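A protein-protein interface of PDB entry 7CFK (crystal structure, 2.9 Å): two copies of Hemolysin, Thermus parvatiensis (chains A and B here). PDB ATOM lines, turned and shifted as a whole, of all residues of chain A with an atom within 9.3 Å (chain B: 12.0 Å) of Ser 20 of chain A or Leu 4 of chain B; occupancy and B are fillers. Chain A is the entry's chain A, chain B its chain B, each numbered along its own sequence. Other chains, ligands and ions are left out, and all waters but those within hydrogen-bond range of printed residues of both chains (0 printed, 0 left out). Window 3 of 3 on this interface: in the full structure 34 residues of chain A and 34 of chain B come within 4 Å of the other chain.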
ATOM      1  N   LEU A  12     -16.665 -27.486   0.997  1.00  0.00           N
ATOM      2  CA  LEU A  12     -17.350 -26.350   0.376  1.00  0.00           C
ATOM      3  C   LEU A  12     -18.854 -26.567   0.214  1.00  0.00           C
ATOM      4  O   LEU A  12     -19.653 -25.639   0.434  1.00  0.00           O
ATOM      5  CB  LEU A  12     -16.694 -26.020  -0.973  1.00  0.00           C
ATOM      6  CG  LEU A  12     -15.404 -25.171  -0.929  1.00  0.00           C
ATOM      7  CD1 LEU A  12     -15.733 -23.747  -0.497  1.00  0.00           C
ATOM      8  CD2 LEU A  12     -14.280 -25.720  -0.032  1.00  0.00           C
ATOM      9  N   ILE A  13     -19.274 -27.785  -0.129  1.00  0.00           N
ATOM     10  CA  ILE A  13     -20.708 -28.050  -0.239  1.00  0.00           C
ATOM     11  C   ILE A  13     -21.386 -28.126   1.120  1.00  0.00           C
ATOM     12  O   ILE A  13     -22.609 -28.010   1.190  1.00  0.00           O
ATOM     13  CB  ILE A  13     -21.000 -29.343  -1.018  1.00  0.00           C
ATOM     14  CG1 ILE A  13     -20.644 -30.562  -0.174  1.00  0.00           C
ATOM     15  CG2 ILE A  13     -20.249 -29.341  -2.332  1.00  0.00           C
ATOM     16  CD1 ILE A  13     -20.838 -31.844  -0.901  1.00  0.00           C
ATOM     17  N   LEU A  14     -20.639 -28.313   2.210  1.00  0.00           N
ATOM     18  CA  LEU A  14     -21.271 -28.205   3.520  1.00  0.00           C
ATOM     19  C   LEU A  14     -21.786 -26.787   3.763  1.00  0.00           C
ATOM     20  O   LEU A  14     -22.943 -26.587   4.168  1.00  0.00           O
ATOM     21  CB  LEU A  14     -20.277 -28.635   4.592  1.00  0.00           C
ATOM     22  CG  LEU A  14     -20.226 -30.157   4.675  1.00  0.00           C
ATOM     23  CD1 LEU A  14     -19.134 -30.655   5.604  1.00  0.00           C
ATOM     24  CD2 LEU A  14     -21.582 -30.653   5.141  1.00  0.00           C
ATOM     25  N   ALA A  15     -20.939 -25.782   3.496  1.00  0.00           N
ATOM     26  CA  ALA A  15     -21.378 -24.392   3.606  1.00  0.00           C
ATOM     27  C   ALA A  15     -22.495 -24.102   2.615  1.00  0.00           C
ATOM     28  O   ALA A  15     -23.488 -23.435   2.957  1.00  0.00           O
ATOM     29  CB  ALA A  15     -20.200 -23.449   3.382  1.00  0.00           C
ATOM     30  N   GLY A  16     -22.365 -24.623   1.386  1.00  0.00           N
ATOM     31  CA  GLY A  16     -23.459 -24.504   0.435  1.00  0.00           C
ATOM     32  C   GLY A  16     -24.762 -25.057   0.984  1.00  0.00           C
ATOM     33  O   GLY A  16     -25.820 -24.432   0.848  1.00  0.00           O
ATOM     34  N   ALA A  17     -24.691 -26.226   1.642  1.00  0.00           N
ATOM     35  CA  ALA A  17     -25.852 -26.871   2.250  1.00  0.00           C
ATOM     36  C   ALA A  17     -26.454 -26.024   3.361  1.00  0.00           C
ATOM     37  O   ALA A  17     -27.665 -26.081   3.600  1.00  0.00           O
ATOM     38  CB  ALA A  17     -25.454 -28.241   2.788  1.00  0.00           C
ATOM     39  N   GLU A  18     -25.630 -25.254   4.067  1.00  0.00           N
ATOM     40  CA  GLU A  18     -26.194 -24.188   4.891  1.00  0.00           C
ATOM     41  C   GLU A  18     -27.014 -23.226   4.031  1.00  0.00           C
ATOM     42  O   GLU A  18     -28.128 -22.825   4.399  1.00  0.00           O
ATOM     43  CB  GLU A  18     -25.104 -23.393   5.608  1.00  0.00           C
ATOM     44  CG  GLU A  18     -25.725 -22.368   6.560  1.00  0.00           C
ATOM     45  CD  GLU A  18     -24.820 -21.203   6.896  1.00  0.00           C
ATOM     46  OE1 GLU A  18     -23.768 -21.032   6.234  1.00  0.00           O
ATOM     47  OE2 GLU A  18     -25.193 -20.432   7.803  1.00  0.00           O
ATOM     48  N   GLU A  19     -26.457 -22.834   2.877  1.00  0.00           N
ATOM     49  CA  GLU A  19     -27.058 -21.768   2.078  1.00  0.00           C
ATOM     50  C   GLU A  19     -28.361 -22.216   1.420  1.00  0.00           C
ATOM     51  O   GLU A  19     -29.296 -21.415   1.279  1.00  0.00           O
ATOM     52  CB  GLU A  19     -26.056 -21.286   1.025  1.00  0.00           C
ATOM     53  CG  GLU A  19     -25.038 -20.260   1.534  1.00  0.00           C
ATOM     54  CD  GLU A  19     -25.673 -19.235   2.447  1.00  0.00           C
ATOM     55  OE1 GLU A  19     -25.540 -19.369   3.686  1.00  0.00           O
ATOM     56  OE2 GLU A  19     -26.311 -18.295   1.924  1.00  0.00           O
ATOM     57  N   SER A  20     -28.441 -23.497   1.008  1.00  0.00           N
ATOM     58  CA  SER A  20     -29.619 -24.104   0.384  1.00  0.00           C
ATOM     59  C   SER A  20     -30.645 -24.600   1.381  1.00  0.00           C
ATOM     60  O   SER A  20     -31.457 -25.466   1.037  1.00  0.00           O
ATOM     61  CB  SER A  20     -29.210 -25.265  -0.516  1.00  0.00           C
ATOM     62  OG  SER A  20     -28.832 -24.797  -1.794  1.00  0.00           O
ATOM     63  N   GLY A  21     -30.612 -24.096   2.610  1.00  0.00           N
ATOM     64  CA  GLY A  21     -31.570 -24.489   3.614  1.00  0.00           C
ATOM     65  C   GLY A  21     -31.469 -25.925   4.066  1.00  0.00           C
ATOM     66  O   GLY A  21     -32.326 -26.363   4.829  1.00  0.00           O
ATOM     67  N   ALA A  22     -30.441 -26.668   3.647  1.00  0.00           N
ATOM     68  CA  ALA A  22     -30.365 -28.089   3.981  1.00  0.00           C
ATOM     69  C   ALA A  22     -29.974 -28.332   5.424  1.00  0.00           C
ATOM     70  O   ALA A  22     -30.359 -29.355   6.000  1.00  0.00           O
ATOM     71  CB  ALA A  22     -29.364 -28.808   3.081  1.00  0.00           C
ATOM     72  N   ILE A  23     -29.185 -27.436   6.010  1.00  0.00           N
ATOM     73  CA  ILE A  23     -28.732 -27.590   7.380  1.00  0.00           C
ATOM     74  C   ILE A  23     -28.788 -26.231   8.069  1.00  0.00           C
ATOM     75  O   ILE A  23     -28.561 -25.189   7.437  1.00  0.00           O
ATOM     76  CB  ILE A  23     -27.319 -28.212   7.437  1.00  0.00           C
ATOM     77  CG1 ILE A  23     -26.335 -27.450   6.562  1.00  0.00           C
ATOM     78  CG2 ILE A  23     -27.350 -29.645   6.934  1.00  0.00           C
ATOM     79  CD1 ILE A  23     -24.917 -27.990   6.668  1.00  0.00           C
ATOM     80  N   GLN A  24     -29.139 -26.254   9.361  1.00  0.00           N
ATOM     81  CA  GLN A  24     -29.112 -25.066  10.199  1.00  0.00           C
ATOM     82  C   GLN A  24     -27.677 -24.593  10.393  1.00  0.00           C
ATOM     83  O   GLN A  24     -26.739 -25.395  10.327  1.00  0.00           O
ATOM     84  CB  GLN A  24     -29.681 -25.354  11.576  1.00  0.00           C
ATOM     85  CG  GLN A  24     -31.113 -25.694  11.640  1.00  0.00           C
ATOM     86  CD  GLN A  24     -31.453 -26.267  12.980  1.00  0.00           C
ATOM     87  OE1 GLN A  24     -31.502 -25.558  13.974  1.00  0.00           O
ATOM     88  NE2 GLN A  24     -31.649 -27.572  13.026  1.00  0.00           N
ATOM     89  N   THR B   2     -20.191 -23.378  -4.261  1.00  0.00           N
ATOM     90  CA  THR B   2     -21.000 -22.948  -5.402  1.00  0.00           C
ATOM     91  C   THR B   2     -22.360 -23.671  -5.532  1.00  0.00           C
ATOM     92  O   THR B   2     -23.388 -23.000  -5.615  1.00  0.00           O
ATOM     93  CB  THR B   2     -20.217 -23.104  -6.736  1.00  0.00           C
ATOM     94  N   PRO B   3     -22.386 -25.010  -5.544  1.00  0.00           N
ATOM     95  CA  PRO B   3     -23.636 -25.716  -5.871  1.00  0.00           C
ATOM     96  C   PRO B   3     -24.712 -25.538  -4.800  1.00  0.00           C
ATOM     97  O   PRO B   3     -24.490 -24.954  -3.732  1.00  0.00           O
ATOM     98  CB  PRO B   3     -23.199 -27.188  -5.985  1.00  0.00           C
ATOM     99  CG  PRO B   3     -21.706 -27.149  -6.123  1.00  0.00           C
ATOM    100  CD  PRO B   3     -21.296 -25.975  -5.296  1.00  0.00           C
ATOM    101  N   LEU B   4     -25.914 -26.044  -5.126  1.00  0.00           N
ATOM    102  CA  LEU B   4     -27.087 -26.039  -4.249  1.00  0.00           C
ATOM    103  C   LEU B   4     -27.573 -27.471  -4.060  1.00  0.00           C
ATOM    104  O   LEU B   4     -27.728 -28.210  -5.039  1.00  0.00           O
ATOM    105  CB  LEU B   4     -28.211 -25.167  -4.827  1.00  0.00           C
ATOM    106  N   VAL B   5     -27.809 -27.866  -2.803  1.00  0.00           N
ATOM    107  CA  VAL B   5     -28.082 -29.259  -2.463  1.00  0.00           C
ATOM    108  C   VAL B   5     -29.066 -29.344  -1.295  1.00  0.00           C
ATOM    109  O   VAL B   5     -29.215 -28.412  -0.499  1.00  0.00           O
ATOM    110  CB  VAL B   5     -26.775 -29.998  -2.111  1.00  0.00           C
ATOM    111  CG1 VAL B   5     -25.908 -30.177  -3.343  1.00  0.00           C
ATOM    112  CG2 VAL B   5     -26.035 -29.222  -1.058  1.00  0.00           C
ATOM    113  N   SER B   6     -29.724 -30.492  -1.186  1.00  0.00           N
ATOM    114  CA  SER B   6     -30.683 -30.765  -0.127  1.00  0.00           C
ATOM    115  C   SER B   6     -30.099 -31.749   0.877  1.00  0.00           C
ATOM    116  O   SER B   6     -29.025 -32.314   0.674  1.00  0.00           O
ATOM    117  CB  SER B   6     -31.979 -31.326  -0.712  1.00  0.00           C
ATOM    118  OG  SER B   6     -31.796 -32.659  -1.169  1.00  0.00           O
ATOM    119  N   GLU B   7     -30.835 -31.965   1.968  1.00  0.00           N
ATOM    120  CA  GLU B   7     -30.338 -32.846   3.025  1.00  0.00           C
ATOM    121  C   GLU B   7     -30.121 -34.269   2.510  1.00  0.00           C
ATOM    122  O   GLU B   7     -29.121 -34.917   2.856  1.00  0.00           O
ATOM    123  CB  GLU B   7     -31.303 -32.840   4.213  1.00  0.00           C
ATOM    124  CG  GLU B   7     -30.807 -33.570   5.447  1.00  0.00           C
ATOM    125  CD  GLU B   7     -31.848 -33.617   6.564  1.00  0.00           C
ATOM    126  OE1 GLU B   7     -31.798 -34.564   7.395  1.00  0.00           O
ATOM    127  OE2 GLU B   7     -32.708 -32.703   6.621  1.00  0.00           O
ATOM    128  N   GLU B   8     -31.043 -34.772   1.680  1.00  0.00           N
ATOM    129  CA  GLU B   8     -30.898 -36.123   1.143  1.00  0.00           C
ATOM    130  C   GLU B   8     -29.700 -36.220   0.206  1.00  0.00           C
ATOM    131  O   GLU B   8     -28.898 -37.163   0.292  1.00  0.00           O
ATOM    132  CB  GLU B   8     -32.179 -36.538   0.426  1.00  0.00           C
ATOM    133  N   GLU B   9     -29.559 -35.247  -0.696  1.00  0.00           N
ATOM    134  CA  GLU B   9     -28.413 -35.244  -1.602  1.00  0.00           C
ATOM    135  C   GLU B   9     -27.098 -35.143  -0.826  1.00  0.00           C
ATOM    136  O   GLU B   9     -26.096 -35.768  -1.197  1.00  0.00           O
ATOM    137  CB  GLU B   9     -28.551 -34.103  -2.622  1.00  0.00           C
ATOM    138  N   LEU B  10     -27.088 -34.373   0.269  1.00  0.00           N
ATOM    139  CA  LEU B  10     -25.872 -34.224   1.067  1.00  0.00           C
ATOM    140  C   LEU B  10     -25.505 -35.538   1.764  1.00  0.00           C
ATOM    141  O   LEU B  10     -24.328 -35.920   1.794  1.00  0.00           O
ATOM    142  CB  LEU B  10     -26.052 -33.055   2.055  1.00  0.00           C
ATOM    143  CG  LEU B  10     -25.130 -32.699   3.229  1.00  0.00           C
ATOM    144  CD1 LEU B  10     -23.835 -32.160   2.714  1.00  0.00           C
ATOM    145  CD2 LEU B  10     -25.766 -31.646   4.101  1.00  0.00           C
ATOM    146  N   LYS B  11     -26.496 -36.269   2.291  1.00  0.00           N
ATOM    147  CA  LYS B  11     -26.199 -37.587   2.857  1.00  0.00           C
ATOM    148  C   LYS B  11     -25.650 -38.540   1.790  1.00  0.00           C
ATOM    149  O   LYS B  11     -24.750 -39.356   2.063  1.00  0.00           O
ATOM    150  CB  LYS B  11     -27.452 -38.169   3.514  1.00  0.00           C
ATOM    151  CG  LYS B  11     -28.063 -37.273   4.583  1.00  0.00           C
ATOM    152  CD  LYS B  11     -29.294 -37.895   5.229  1.00  0.00           C
ATOM    153  CE  LYS B  11     -29.790 -37.056   6.405  1.00  0.00           C
ATOM    154  NZ  LYS B  11     -30.920 -37.695   7.158  1.00  0.00           N
ATOM    155  N   LEU B  12     -26.179 -38.450   0.560  1.00  0.00           N
ATOM    156  CA  LEU B  12     -25.664 -39.284  -0.531  1.00  0.00           C
ATOM    157  C   LEU B  12     -24.216 -38.928  -0.883  1.00  0.00           C
ATOM    158  O   LEU B  12     -23.382 -39.819  -1.102  1.00  0.00           O
ATOM    159  CB  LEU B  12     -26.572 -39.162  -1.760  1.00  0.00           C
ATOM    160  CG  LEU B  12     -27.847 -40.012  -1.778  1.00  0.00           C
ATOM    161  CD1 LEU B  12     -28.893 -39.400  -2.701  1.00  0.00           C
ATOM    162  CD2 LEU B  12     -27.527 -41.440  -2.194  1.00  0.00           C
ATOM    163  N   ILE B  13     -23.898 -37.632  -0.947  1.00  0.00           N
ATOM    164  CA  ILE B  13     -22.516 -37.234  -1.208  1.00  0.00           C
ATOM    165  C   ILE B  13     -21.604 -37.693  -0.076  1.00  0.00           C
ATOM    166  O   ILE B  13     -20.428 -38.001  -0.303  1.00  0.00           O
ATOM    167  CB  ILE B  13     -22.399 -35.711  -1.435  1.00  0.00           C
ATOM    168  CG1 ILE B  13     -23.405 -35.228  -2.470  1.00  0.00           C
ATOM    169  CG2 ILE B  13     -20.992 -35.342  -1.901  1.00  0.00           C
ATOM    170  CD1 ILE B  13     -23.280 -33.757  -2.781  1.00  0.00           C
ATOM    171  N   LEU B  35     -26.468 -35.357  11.547  1.00  0.00           N
ATOM    172  CA  LEU B  35     -27.661 -35.154  10.723  1.00  0.00           C
ATOM    173  C   LEU B  35     -28.853 -35.971  11.222  1.00  0.00           C
ATOM    174  O   LEU B  35     -29.998 -35.508  11.169  1.00  0.00           O
ATOM    175  CB  LEU B  35     -27.354 -35.495   9.266  1.00  0.00           C
ATOM    176  CG  LEU B  35     -26.434 -34.497   8.572  1.00  0.00           C
ATOM    177  CD1 LEU B  35     -26.060 -35.014   7.211  1.00  0.00           C
ATOM    178  CD2 LEU B  35     -27.112 -33.156   8.470  1.00  0.00           C
ATOM    179  N   GLU B  38     -31.657 -34.983  14.525  1.00  0.00           N
ATOM    180  CA  GLU B  38     -32.984 -34.384  14.428  1.00  0.00           C
ATOM    181  C   GLU B  38     -34.077 -35.428  14.192  1.00  0.00           C
ATOM    182  O   GLU B  38     -35.263 -35.127  14.359  1.00  0.00           O
ATOM    183  CB  GLU B  38     -33.006 -33.352  13.303  1.00  0.00           C
ATOM    184  CG  GLU B  38     -33.250 -33.984  11.937  1.00  0.00           C
ATOM    185  CD  GLU B  38     -33.597 -32.984  10.877  1.00  0.00           C
ATOM    186  OE1 GLU B  38     -32.857 -31.993  10.732  1.00  0.00           O
ATOM    187  OE2 GLU B  38     -34.627 -33.179  10.205  1.00  0.00           O
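O of Ala 17 of chain A is in hydrogen-bond range of N of Ala 22 of chain A (2.8 Å). The side-chain carboxylate (OE1) of Glu 7 of chain B lies within salt-bridge range of the side-chain amino group (NZ) of Lys 11 of chain B. O of Ala 17 of chain A lies within hydrogen-bond range of N of Ile 23 of chain A (3.2 Å). The side-chain hydroxyl (OG) of Ser 6 of chain B sits at hydrogen-bond distance from the backbone NH (N) of Glu 9 of chain B (3.5 Å).
Ile 13 of chain B touches its own counterpart, Ile 13 of chain A. Positions printed for both chains: 12 and 13. Of the 10 pairs that touch across the chains among the printed residues, 1 has its exchanged pair printed and touching as well.
Of the 14 printed residues of chain B, 7 touch a printed residue of chain A. Hydrophobic or aromatic side chains of chain B that line the printed part of chain A: Leu 4, Leu 10, Ile 13 and Leu 35. Among the printed residues, 10 pairs touch across the chains. Among the printed residues, no Asp or Glu carboxylate lies within 4 Å of a Lys or Arg side-chain nitrogen of the other chain.
CD1 of Ile 13 of chain B touches CD1 of Ile 13 of chain A, at 3.6 Å. Leu 14 of chain A touches Leu 10 of chain B. CD2 of Leu 10 of chain B touches CB of Ala 17 of chain A, 3.7 Å away. OG of Ser 20 of chain A touches CB of Leu 4 of chain B, at 3.1 Å. CB of Ala 22 of chain A touches O of Val 5 of chain B (3.6 Å). Ala 22 of chain A touches Ser 6 of chain B. Glu 7 of chain B touches Ala 22 of chain A (N to CB, 3.7 Å). Ile 23 of chain A touches Leu 10 of chain B. Ile 23 of chain A touches Leu 35 of chain B (CG2 to CD2, 3.8 Å).
N of Val 5 of chain B lies within hydrogen-bond range of OG of Ser 20 of chain A.
Of the printed residues of chain B, Ile 13 of chain A touches Ile 13 (3.6 Å). No residue of chain B comes within 4 Å of Glu 19 of chain A. Of chain B, only Leu 4 (3.1 Å) and Val 5 (3.1 Å) come within 4 Å of Ser 20 of chain A. Gly 21 of chain A touches none of the printed residues of chain B. Ala 22 of chain A touches just these residues of chain B: Val 5, Ser 6 and Glu 7. Thr 2 of chain B touches none of the printed residues of chain A. Of chain A, only Ser 20 (3.1 Å) comes within 4 Å of Leu 4 of chain B. Of the printed residues of chain A, Val 5 of chain B touches Ser 20 (3.1 Å) and Ala 22 (3.6 Å). Leu 12 of chain B touches none of the printed residues of chain A. Printed residues of chain A within 4 Å of Leu 35 of chain B: Ile 23 (3.8 Å). The nearest residue of chain A that does not touch Leu 4 of chain B is Gly 16 of chain A (5.5 Å). The nearest printed residue of chain B that does not touch Ile 13 of chain A is Val 5 of chain B (4.3 Å).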
